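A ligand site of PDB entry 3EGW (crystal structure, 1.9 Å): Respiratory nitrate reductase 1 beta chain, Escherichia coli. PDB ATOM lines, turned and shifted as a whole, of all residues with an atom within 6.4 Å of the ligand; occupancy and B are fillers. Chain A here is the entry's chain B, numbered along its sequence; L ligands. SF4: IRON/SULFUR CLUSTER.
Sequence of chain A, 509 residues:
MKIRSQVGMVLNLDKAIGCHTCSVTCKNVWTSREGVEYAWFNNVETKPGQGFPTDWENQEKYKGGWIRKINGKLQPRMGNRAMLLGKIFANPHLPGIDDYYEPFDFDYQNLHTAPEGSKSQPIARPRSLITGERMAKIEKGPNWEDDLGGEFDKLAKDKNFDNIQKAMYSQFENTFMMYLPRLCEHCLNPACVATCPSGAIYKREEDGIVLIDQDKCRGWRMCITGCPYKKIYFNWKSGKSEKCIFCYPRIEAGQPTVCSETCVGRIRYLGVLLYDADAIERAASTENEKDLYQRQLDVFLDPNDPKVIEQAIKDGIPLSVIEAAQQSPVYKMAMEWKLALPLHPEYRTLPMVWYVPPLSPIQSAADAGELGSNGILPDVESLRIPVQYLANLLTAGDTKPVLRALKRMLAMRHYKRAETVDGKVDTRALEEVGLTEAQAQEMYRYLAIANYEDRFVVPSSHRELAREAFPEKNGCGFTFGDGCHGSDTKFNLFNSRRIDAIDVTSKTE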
ATOM      1  N   MET A   9       4.701 -38.691  12.018  1.00  0.00           N
ATOM      2  CA  MET A   9       5.789 -38.065  12.743  1.00  0.00           C
ATOM      3  C   MET A   9       5.537 -38.103  14.242  1.00  0.00           C
ATOM      4  O   MET A   9       4.395 -37.983  14.703  1.00  0.00           O
ATOM      5  CB  MET A   9       5.962 -36.597  12.323  1.00  0.00           C
ATOM      6  CG  MET A   9       7.120 -35.883  13.030  1.00  0.00           C
ATOM      7  SD  MET A   9       7.106 -34.067  12.782  1.00  0.00           S
ATOM      8  CE  MET A   9       7.649 -33.955  11.073  1.00  0.00           C
ATOM      9  N   CYS A  22      13.682 -25.458  13.869  1.00  0.00           N
ATOM     10  CA  CYS A  22      12.712 -26.048  12.949  1.00  0.00           C
ATOM     11  C   CYS A  22      11.856 -24.967  12.275  1.00  0.00           C
ATOM     12  O   CYS A  22      11.526 -25.065  11.086  1.00  0.00           O
ATOM     13  CB  CYS A  22      11.802 -27.014  13.716  1.00  0.00           C
ATOM     14  SG  CYS A  22      11.148 -26.350  15.285  1.00  0.00           S
ATOM     15  N   THR A  25      14.182 -22.756   9.631  1.00  0.00           N
ATOM     16  CA  THR A  25      14.476 -23.428   8.374  1.00  0.00           C
ATOM     17  C   THR A  25      13.228 -23.522   7.485  1.00  0.00           C
ATOM     18  O   THR A  25      13.301 -23.259   6.290  1.00  0.00           O
ATOM     19  CB  THR A  25      15.097 -24.817   8.594  1.00  0.00           C
ATOM     20  OG1 THR A  25      14.240 -25.627   9.407  1.00  0.00           O
ATOM     21  CG2 THR A  25      16.458 -24.674   9.286  1.00  0.00           C
ATOM     22  N   CYS A  26      12.079 -23.883   8.071  1.00  0.00           N
ATOM     23  CA  CYS A  26      10.846 -23.963   7.272  1.00  0.00           C
ATOM     24  C   CYS A  26      10.537 -22.609   6.659  1.00  0.00           C
ATOM     25  O   CYS A  26      10.205 -22.516   5.468  1.00  0.00           O
ATOM     26  CB  CYS A  26       9.650 -24.391   8.138  1.00  0.00           C
ATOM     27  SG  CYS A  26       8.076 -24.523   7.200  1.00  0.00           S
ATOM     28  N   LYS A  27      10.626 -21.565   7.481  1.00  0.00           N
ATOM     29  CA  LYS A  27      10.346 -20.206   7.030  1.00  0.00           C
ATOM     30  C   LYS A  27      11.218 -19.795   5.843  1.00  0.00           C
ATOM     31  O   LYS A  27      10.707 -19.296   4.841  1.00  0.00           O
ATOM     32  CB  LYS A  27      10.535 -19.212   8.183  1.00  0.00           C
ATOM     33  CG  LYS A  27      10.538 -17.757   7.773  1.00  0.00           C
ATOM     34  CD  LYS A  27       9.234 -17.339   7.111  1.00  0.00           C
ATOM     35  CE  LYS A  27       8.064 -17.355   8.093  1.00  0.00           C
ATOM     36  NZ  LYS A  27       6.802 -16.873   7.437  1.00  0.00           N
ATOM     37  N   TRP A  30      10.054 -22.206   2.711  1.00  0.00           N
ATOM     38  CA  TRP A  30       8.673 -22.107   2.230  1.00  0.00           C
ATOM     39  C   TRP A  30       7.814 -20.861   2.386  1.00  0.00           C
ATOM     40  O   TRP A  30       6.895 -20.668   1.586  1.00  0.00           O
ATOM     41  CB  TRP A  30       7.873 -23.278   2.799  1.00  0.00           C
ATOM     42  CG  TRP A  30       8.539 -24.603   2.635  1.00  0.00           C
ATOM     43  CD1 TRP A  30       9.006 -25.419   3.628  1.00  0.00           C
ATOM     44  CD2 TRP A  30       8.768 -25.299   1.400  1.00  0.00           C
ATOM     45  NE1 TRP A  30       9.522 -26.581   3.081  1.00  0.00           N
ATOM     46  CE2 TRP A  30       9.381 -26.528   1.722  1.00  0.00           C
ATOM     47  CE3 TRP A  30       8.522 -24.988   0.052  1.00  0.00           C
ATOM     48  CZ2 TRP A  30       9.748 -27.464   0.743  1.00  0.00           C
ATOM     49  CZ3 TRP A  30       8.877 -25.913  -0.921  1.00  0.00           C
ATOM     50  CH2 TRP A  30       9.482 -27.142  -0.566  1.00  0.00           C
ATOM     51  N   PHE A  41       4.434 -22.260   9.112  1.00  0.00           N
ATOM     52  CA  PHE A  41       3.964 -23.627   8.901  1.00  0.00           C
ATOM     53  C   PHE A  41       4.339 -24.482  10.108  1.00  0.00           C
ATOM     54  O   PHE A  41       3.554 -25.297  10.582  1.00  0.00           O
ATOM     55  CB  PHE A  41       4.563 -24.216   7.622  1.00  0.00           C
ATOM     56  CG  PHE A  41       3.980 -23.652   6.340  1.00  0.00           C
ATOM     57  CD1 PHE A  41       4.527 -24.012   5.107  1.00  0.00           C
ATOM     58  CD2 PHE A  41       2.890 -22.788   6.359  1.00  0.00           C
ATOM     59  CE1 PHE A  41       3.994 -23.518   3.911  1.00  0.00           C
ATOM     60  CE2 PHE A  41       2.338 -22.294   5.173  1.00  0.00           C
ATOM     61  CZ  PHE A  41       2.892 -22.658   3.946  1.00  0.00           C
ATOM     62  N   ASN A  42       5.564 -24.276  10.597  1.00  0.00           N
ATOM     63  CA  ASN A  42       6.057 -24.947  11.791  1.00  0.00           C
ATOM     64  C   ASN A  42       6.229 -23.800  12.772  1.00  0.00           C
ATOM     65  O   ASN A  42       6.836 -22.792  12.431  1.00  0.00           O
ATOM     66  CB  ASN A  42       7.422 -25.591  11.542  1.00  0.00           C
ATOM     67  CG  ASN A  42       7.992 -26.240  12.797  1.00  0.00           C
ATOM     68  OD1 ASN A  42       7.931 -27.467  12.957  1.00  0.00           O
ATOM     69  ND2 ASN A  42       8.547 -25.429  13.693  1.00  0.00           N
ATOM     70  N   ASN A  43       5.674 -23.922  13.964  1.00  0.00           N
ATOM     71  CA  ASN A  43       5.855 -22.876  14.970  1.00  0.00           C
ATOM     72  C   ASN A  43       5.995 -23.568  16.313  1.00  0.00           C
ATOM     73  O   ASN A  43       5.440 -24.645  16.514  1.00  0.00           O
ATOM     74  CB  ASN A  43       4.663 -21.900  14.998  1.00  0.00           C
ATOM     75  CG  ASN A  43       3.477 -22.424  15.789  1.00  0.00           C
ATOM     76  OD1 ASN A  43       2.813 -23.368  15.379  1.00  0.00           O
ATOM     77  ND2 ASN A  43       3.210 -21.791  16.932  1.00  0.00           N
ATOM     78  N   ARG A 182       4.930 -27.500  16.602  1.00  0.00           N
ATOM     79  CA  ARG A 182       3.883 -28.144  15.840  1.00  0.00           C
ATOM     80  C   ARG A 182       3.775 -27.662  14.416  1.00  0.00           C
ATOM     81  O   ARG A 182       4.210 -26.565  14.053  1.00  0.00           O
ATOM     82  CB  ARG A 182       2.551 -28.013  16.566  1.00  0.00           C
ATOM     83  CG  ARG A 182       2.121 -26.613  16.770  1.00  0.00           C
ATOM     84  CD  ARG A 182       1.037 -26.494  17.830  1.00  0.00           C
ATOM     85  NE  ARG A 182       0.421 -25.171  17.690  1.00  0.00           N
ATOM     86  CZ  ARG A 182      -0.542 -24.896  16.823  1.00  0.00           C
ATOM     87  NH1 ARG A 182      -1.019 -25.848  16.033  1.00  0.00           N
ATOM     88  NH2 ARG A 182      -0.988 -23.654  16.717  1.00  0.00           N
ATOM     89  N   LEU A 183       3.196 -28.529  13.591  1.00  0.00           N
ATOM     90  CA  LEU A 183       3.010 -28.268  12.190  1.00  0.00           C
ATOM     91  C   LEU A 183       1.637 -28.833  11.859  1.00  0.00           C
ATOM     92  O   LEU A 183       0.838 -29.105  12.761  1.00  0.00           O
ATOM     93  CB  LEU A 183       4.084 -29.000  11.389  1.00  0.00           C
ATOM     94  CG  LEU A 183       4.250 -30.506  11.675  1.00  0.00           C
ATOM     95  CD1 LEU A 183       4.845 -31.183  10.452  1.00  0.00           C
ATOM     96  CD2 LEU A 183       5.121 -30.714  12.903  1.00  0.00           C
ATOM     97  N   CYS A 184       1.352 -29.014  10.571  1.00  0.00           N
ATOM     98  CA  CYS A 184       0.075 -29.591  10.183  1.00  0.00           C
ATOM     99  C   CYS A 184       0.125 -31.070  10.590  1.00  0.00           C
ATOM    100  O   CYS A 184       1.170 -31.708  10.482  1.00  0.00           O
ATOM    101  CB  CYS A 184      -0.120 -29.452   8.674  1.00  0.00           C
ATOM    102  SG  CYS A 184      -1.389 -30.523   7.988  1.00  0.00           S
ATOM    103  N   HIS A 186      -1.608 -33.482   9.158  1.00  0.00           N
ATOM    104  CA  HIS A 186      -1.876 -34.312   7.979  1.00  0.00           C
ATOM    105  C   HIS A 186      -2.785 -35.475   8.379  1.00  0.00           C
ATOM    106  O   HIS A 186      -2.493 -36.653   8.130  1.00  0.00           O
ATOM    107  CB  HIS A 186      -0.556 -34.780   7.378  1.00  0.00           C
ATOM    108  CG  HIS A 186       0.257 -33.657   6.810  1.00  0.00           C
ATOM    109  ND1 HIS A 186       0.048 -33.155   5.542  1.00  0.00           N
ATOM    110  CD2 HIS A 186       1.189 -32.849   7.380  1.00  0.00           C
ATOM    111  CE1 HIS A 186       0.805 -32.086   5.363  1.00  0.00           C
ATOM    112  NE2 HIS A 186       1.510 -31.876   6.464  1.00  0.00           N
ATOM    113  N   LYS A 243      -0.445 -24.068   3.492  1.00  0.00           N
ATOM    114  CA  LYS A 243      -0.219 -24.821   4.709  1.00  0.00           C
ATOM    115  C   LYS A 243       1.023 -25.680   4.578  1.00  0.00           C
ATOM    116  O   LYS A 243       1.558 -25.870   3.484  1.00  0.00           O
ATOM    117  CB  LYS A 243      -1.404 -25.750   4.963  1.00  0.00           C
ATOM    118  CG  LYS A 243      -1.602 -26.770   3.823  1.00  0.00           C
ATOM    119  CD  LYS A 243      -2.793 -27.696   4.047  1.00  0.00           C
ATOM    120  CE  LYS A 243      -2.585 -28.646   5.212  1.00  0.00           C
ATOM    121  NZ  LYS A 243      -1.437 -29.583   4.981  1.00  0.00           N
ATOM    122  N   CYS A 244       1.475 -26.213   5.706  1.00  0.00           N
ATOM    123  CA  CYS A 244       2.613 -27.121   5.738  1.00  0.00           C
ATOM    124  C   CYS A 244       2.363 -28.142   4.636  1.00  0.00           C
ATOM    125  O   CYS A 244       1.259 -28.683   4.535  1.00  0.00           O
ATOM    126  CB  CYS A 244       2.652 -27.813   7.095  1.00  0.00           C
ATOM    127  SG  CYS A 244       3.585 -29.339   7.140  1.00  0.00           S
ATOM    128  N   ILE A 245       3.368 -28.408   3.802  1.00  0.00           N
ATOM    129  CA  ILE A 245       3.227 -29.377   2.716  1.00  0.00           C
ATOM    130  C   ILE A 245       3.997 -30.666   3.029  1.00  0.00           C
ATOM    131  O   ILE A 245       4.238 -31.490   2.156  1.00  0.00           O
ATOM    132  CB  ILE A 245       3.757 -28.797   1.370  1.00  0.00           C
ATOM    133  CG1 ILE A 245       5.253 -28.482   1.465  1.00  0.00           C
ATOM    134  CG2 ILE A 245       2.983 -27.522   1.013  1.00  0.00           C
ATOM    135  CD1 ILE A 245       5.868 -28.020   0.134  1.00  0.00           C
ATOM    136  N   PHE A 246       4.358 -30.823   4.304  1.00  0.00           N
ATOM    137  CA  PHE A 246       5.134 -31.962   4.791  1.00  0.00           C
ATOM    138  C   PHE A 246       6.354 -32.171   3.890  1.00  0.00           C
ATOM    139  O   PHE A 246       6.793 -33.301   3.673  1.00  0.00           O
ATOM    140  CB  PHE A 246       4.299 -33.239   4.819  1.00  0.00           C
ATOM    141  CG  PHE A 246       4.729 -34.200   5.893  1.00  0.00           C
ATOM    142  CD1 PHE A 246       4.573 -33.877   7.234  1.00  0.00           C
ATOM    143  CD2 PHE A 246       5.326 -35.416   5.561  1.00  0.00           C
ATOM    144  CE1 PHE A 246       4.989 -34.751   8.240  1.00  0.00           C
ATOM    145  CE2 PHE A 246       5.753 -36.301   6.560  1.00  0.00           C
ATOM    146  CZ  PHE A 246       5.592 -35.966   7.900  1.00  0.00           C
ATOM    147  N   CYS A 247       6.888 -31.072   3.374  1.00  0.00           N
ATOM    148  CA  CYS A 247       8.052 -31.146   2.509  1.00  0.00           C
ATOM    149  C   CYS A 247       7.957 -32.280   1.499  1.00  0.00           C
ATOM    150  O   CYS A 247       8.936 -33.007   1.299  1.00  0.00           O
ATOM    151  CB  CYS A 247       9.306 -31.322   3.347  1.00  0.00           C
ATOM    152  SG  CYS A 247       9.756 -29.841   4.251  1.00  0.00           S
ATOM    153  N   TYR A 248       6.804 -32.434   0.859  1.00  0.00           N
ATOM    154  CA  TYR A 248       6.655 -33.530  -0.095  1.00  0.00           C
ATOM    155  C   TYR A 248       7.750 -33.615  -1.166  1.00  0.00           C
ATOM    156  O   TYR A 248       8.091 -34.713  -1.589  1.00  0.00           O
ATOM    157  CB  TYR A 248       5.252 -33.532  -0.727  1.00  0.00           C
ATOM    158  CG  TYR A 248       4.907 -32.393  -1.664  1.00  0.00           C
ATOM    159  CD1 TYR A 248       5.290 -32.432  -3.005  1.00  0.00           C
ATOM    160  CD2 TYR A 248       4.144 -31.318  -1.231  1.00  0.00           C
ATOM    161  CE1 TYR A 248       4.920 -31.406  -3.895  1.00  0.00           C
ATOM    162  CE2 TYR A 248       3.765 -30.286  -2.101  1.00  0.00           C
ATOM    163  CZ  TYR A 248       4.155 -30.344  -3.428  1.00  0.00           C
ATOM    164  OH  TYR A 248       3.783 -29.331  -4.285  1.00  0.00           O
ATOM    165  N   THR A 257      11.691 -34.437   6.331  1.00  0.00           N
ATOM    166  CA  THR A 257      11.185 -33.096   6.074  1.00  0.00           C
ATOM    167  C   THR A 257      12.290 -32.166   6.557  1.00  0.00           C
ATOM    168  O   THR A 257      13.194 -32.587   7.273  1.00  0.00           O
ATOM    169  CB  THR A 257       9.904 -32.791   6.886  1.00  0.00           C
ATOM    170  OG1 THR A 257      10.244 -32.677   8.276  1.00  0.00           O
ATOM    171  CG2 THR A 257       8.865 -33.895   6.706  1.00  0.00           C
ATOM    172  N   VAL A 258      12.231 -30.897   6.152  1.00  0.00           N
ATOM    173  CA  VAL A 258      13.246 -29.939   6.573  1.00  0.00           C
ATOM    174  C   VAL A 258      13.241 -29.775   8.096  1.00  0.00           C
ATOM    175  O   VAL A 258      14.307 -29.804   8.722  1.00  0.00           O
ATOM    176  CB  VAL A 258      13.014 -28.558   5.922  1.00  0.00           C
ATOM    177  CG1 VAL A 258      13.937 -27.517   6.557  1.00  0.00           C
ATOM    178  CG2 VAL A 258      13.310 -28.641   4.418  1.00  0.00           C
ATOM    179  N   CYS A 259      12.058 -29.612   8.699  1.00  0.00           N
ATOM    180  CA  CYS A 259      11.986 -29.444  10.147  1.00  0.00           C
ATOM    181  C   CYS A 259      12.421 -30.694  10.914  1.00  0.00           C
ATOM    182  O   CYS A 259      12.811 -30.605  12.083  1.00  0.00           O
ATOM    183  CB  CYS A 259      10.572 -29.022  10.593  1.00  0.00           C
ATOM    184  SG  CYS A 259       9.207 -30.111  10.123  1.00  0.00           S
ATOM    185  N   SER A 260      12.357 -31.848  10.264  1.00  0.00           N
ATOM    186  CA  SER A 260      12.776 -33.093  10.919  1.00  0.00           C
ATOM    187  C   SER A 260      14.300 -33.246  10.888  1.00  0.00           C
ATOM    188  O   SER A 260      14.917 -33.515  11.915  1.00  0.00           O
ATOM    189  CB  SER A 260      12.129 -34.296  10.228  1.00  0.00           C
ATOM    190  OG  SER A 260      10.739 -34.326  10.486  1.00  0.00           O
ATOM    191  N   ARG A 268      12.513 -35.411  16.664  1.00  0.00           N
ATOM    192  CA  ARG A 268      11.554 -35.816  15.637  1.00  0.00           C
ATOM    193  C   ARG A 268      11.869 -37.129  14.935  1.00  0.00           C
ATOM    194  O   ARG A 268      12.996 -37.353  14.492  1.00  0.00           O
ATOM    195  CB  ARG A 268      11.396 -34.697  14.595  1.00  0.00           C
ATOM    196  CG  ARG A 268      11.067 -33.359  15.216  1.00  0.00           C
ATOM    197  CD  ARG A 268      10.461 -32.401  14.212  1.00  0.00           C
ATOM    198  NE  ARG A 268      10.176 -31.107  14.831  1.00  0.00           N
ATOM    199  CZ  ARG A 268       9.404 -30.171  14.293  1.00  0.00           C
ATOM    200  NH1 ARG A 268       8.822 -30.384  13.118  1.00  0.00           N
ATOM    201  NH2 ARG A 268       9.220 -29.019  14.920  1.00  0.00           N
HETATM  202 FE1  SF4 L   1       8.181 -29.101   5.779  1.00  0.00          FE
HETATM  203 FE2  SF4 L   1       5.809 -28.769   7.058  1.00  0.00          FE
HETATM  204 FE3  SF4 L   1       8.101 -29.048   8.424  1.00  0.00          FE
HETATM  205 FE4  SF4 L   1       7.605 -26.764   7.063  1.00  0.00          FE
HETATM  206  S1  SF4 L   1       6.452 -27.544   8.851  1.00  0.00           S
HETATM  207  S2  SF4 L   1       9.545 -27.917   7.140  1.00  0.00           S
HETATM  208  S3  SF4 L   1       6.528 -27.611   5.226  1.00  0.00           S
HETATM  209  S4  SF4 L   1       7.144 -30.623   7.098  1.00  0.00           S
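N of Cys 259 sits close to S2 of the ligand, at 3.4 Å. FE3 of the ligand is bound by SG of Cys 259 (2.3 Å). An iron atom (FE4) of the ligand is bound by the side-chain sulfur (SG) of Cys 26. The side-chain sulfur (SG) of Cys 244 is bound to an iron atom (FE2) of the ligand, 2.3 Å away. A sulfur (S4) of the ligand lies close to the backbone NH (N) of Cys 247, 3.8 Å away. SG of Cys 247 binds FE1 of the ligand, at 2.3 Å. S3 of the ligand lies close to N of Ile 245, 3.6 Å away.
OG1 of Thr 257 lies close to SG of Cys 259 (3.3 Å). The guanidinium group (NH1) of Arg 268 sits close to the side-chain sulfur (SG) of Cys 259 (3.0 Å). SG of Cys 244 sits close to N of Phe 246 (3.3 Å). The indole nitrogen of Trp 30 sits close to the side-chain sulfur of Cys 247 (3.5 Å). The side-chain sulfur (SG) of Cys 247 lies close to the backbone NH (N) of Val 258 (3.3 Å). OD1 of Asn 42 is in hydrogen-bond range of NH2 of Arg 268 (2.8 Å). ND2 of Asn 42 sits close to SG of Cys 22. OG1 of Thr 257 sits at hydrogen-bond distance from OG of Ser 260, at 2.8 Å.
Residues that only touch the ligand: Phe 246, Asn 42, Thr 257, Trp 30, Val 258, Leu 183 and Phe 41. Hydrophobic or aromatic side chains within 4 Å of the ligand: Trp 30, Leu 183 and Val 258.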
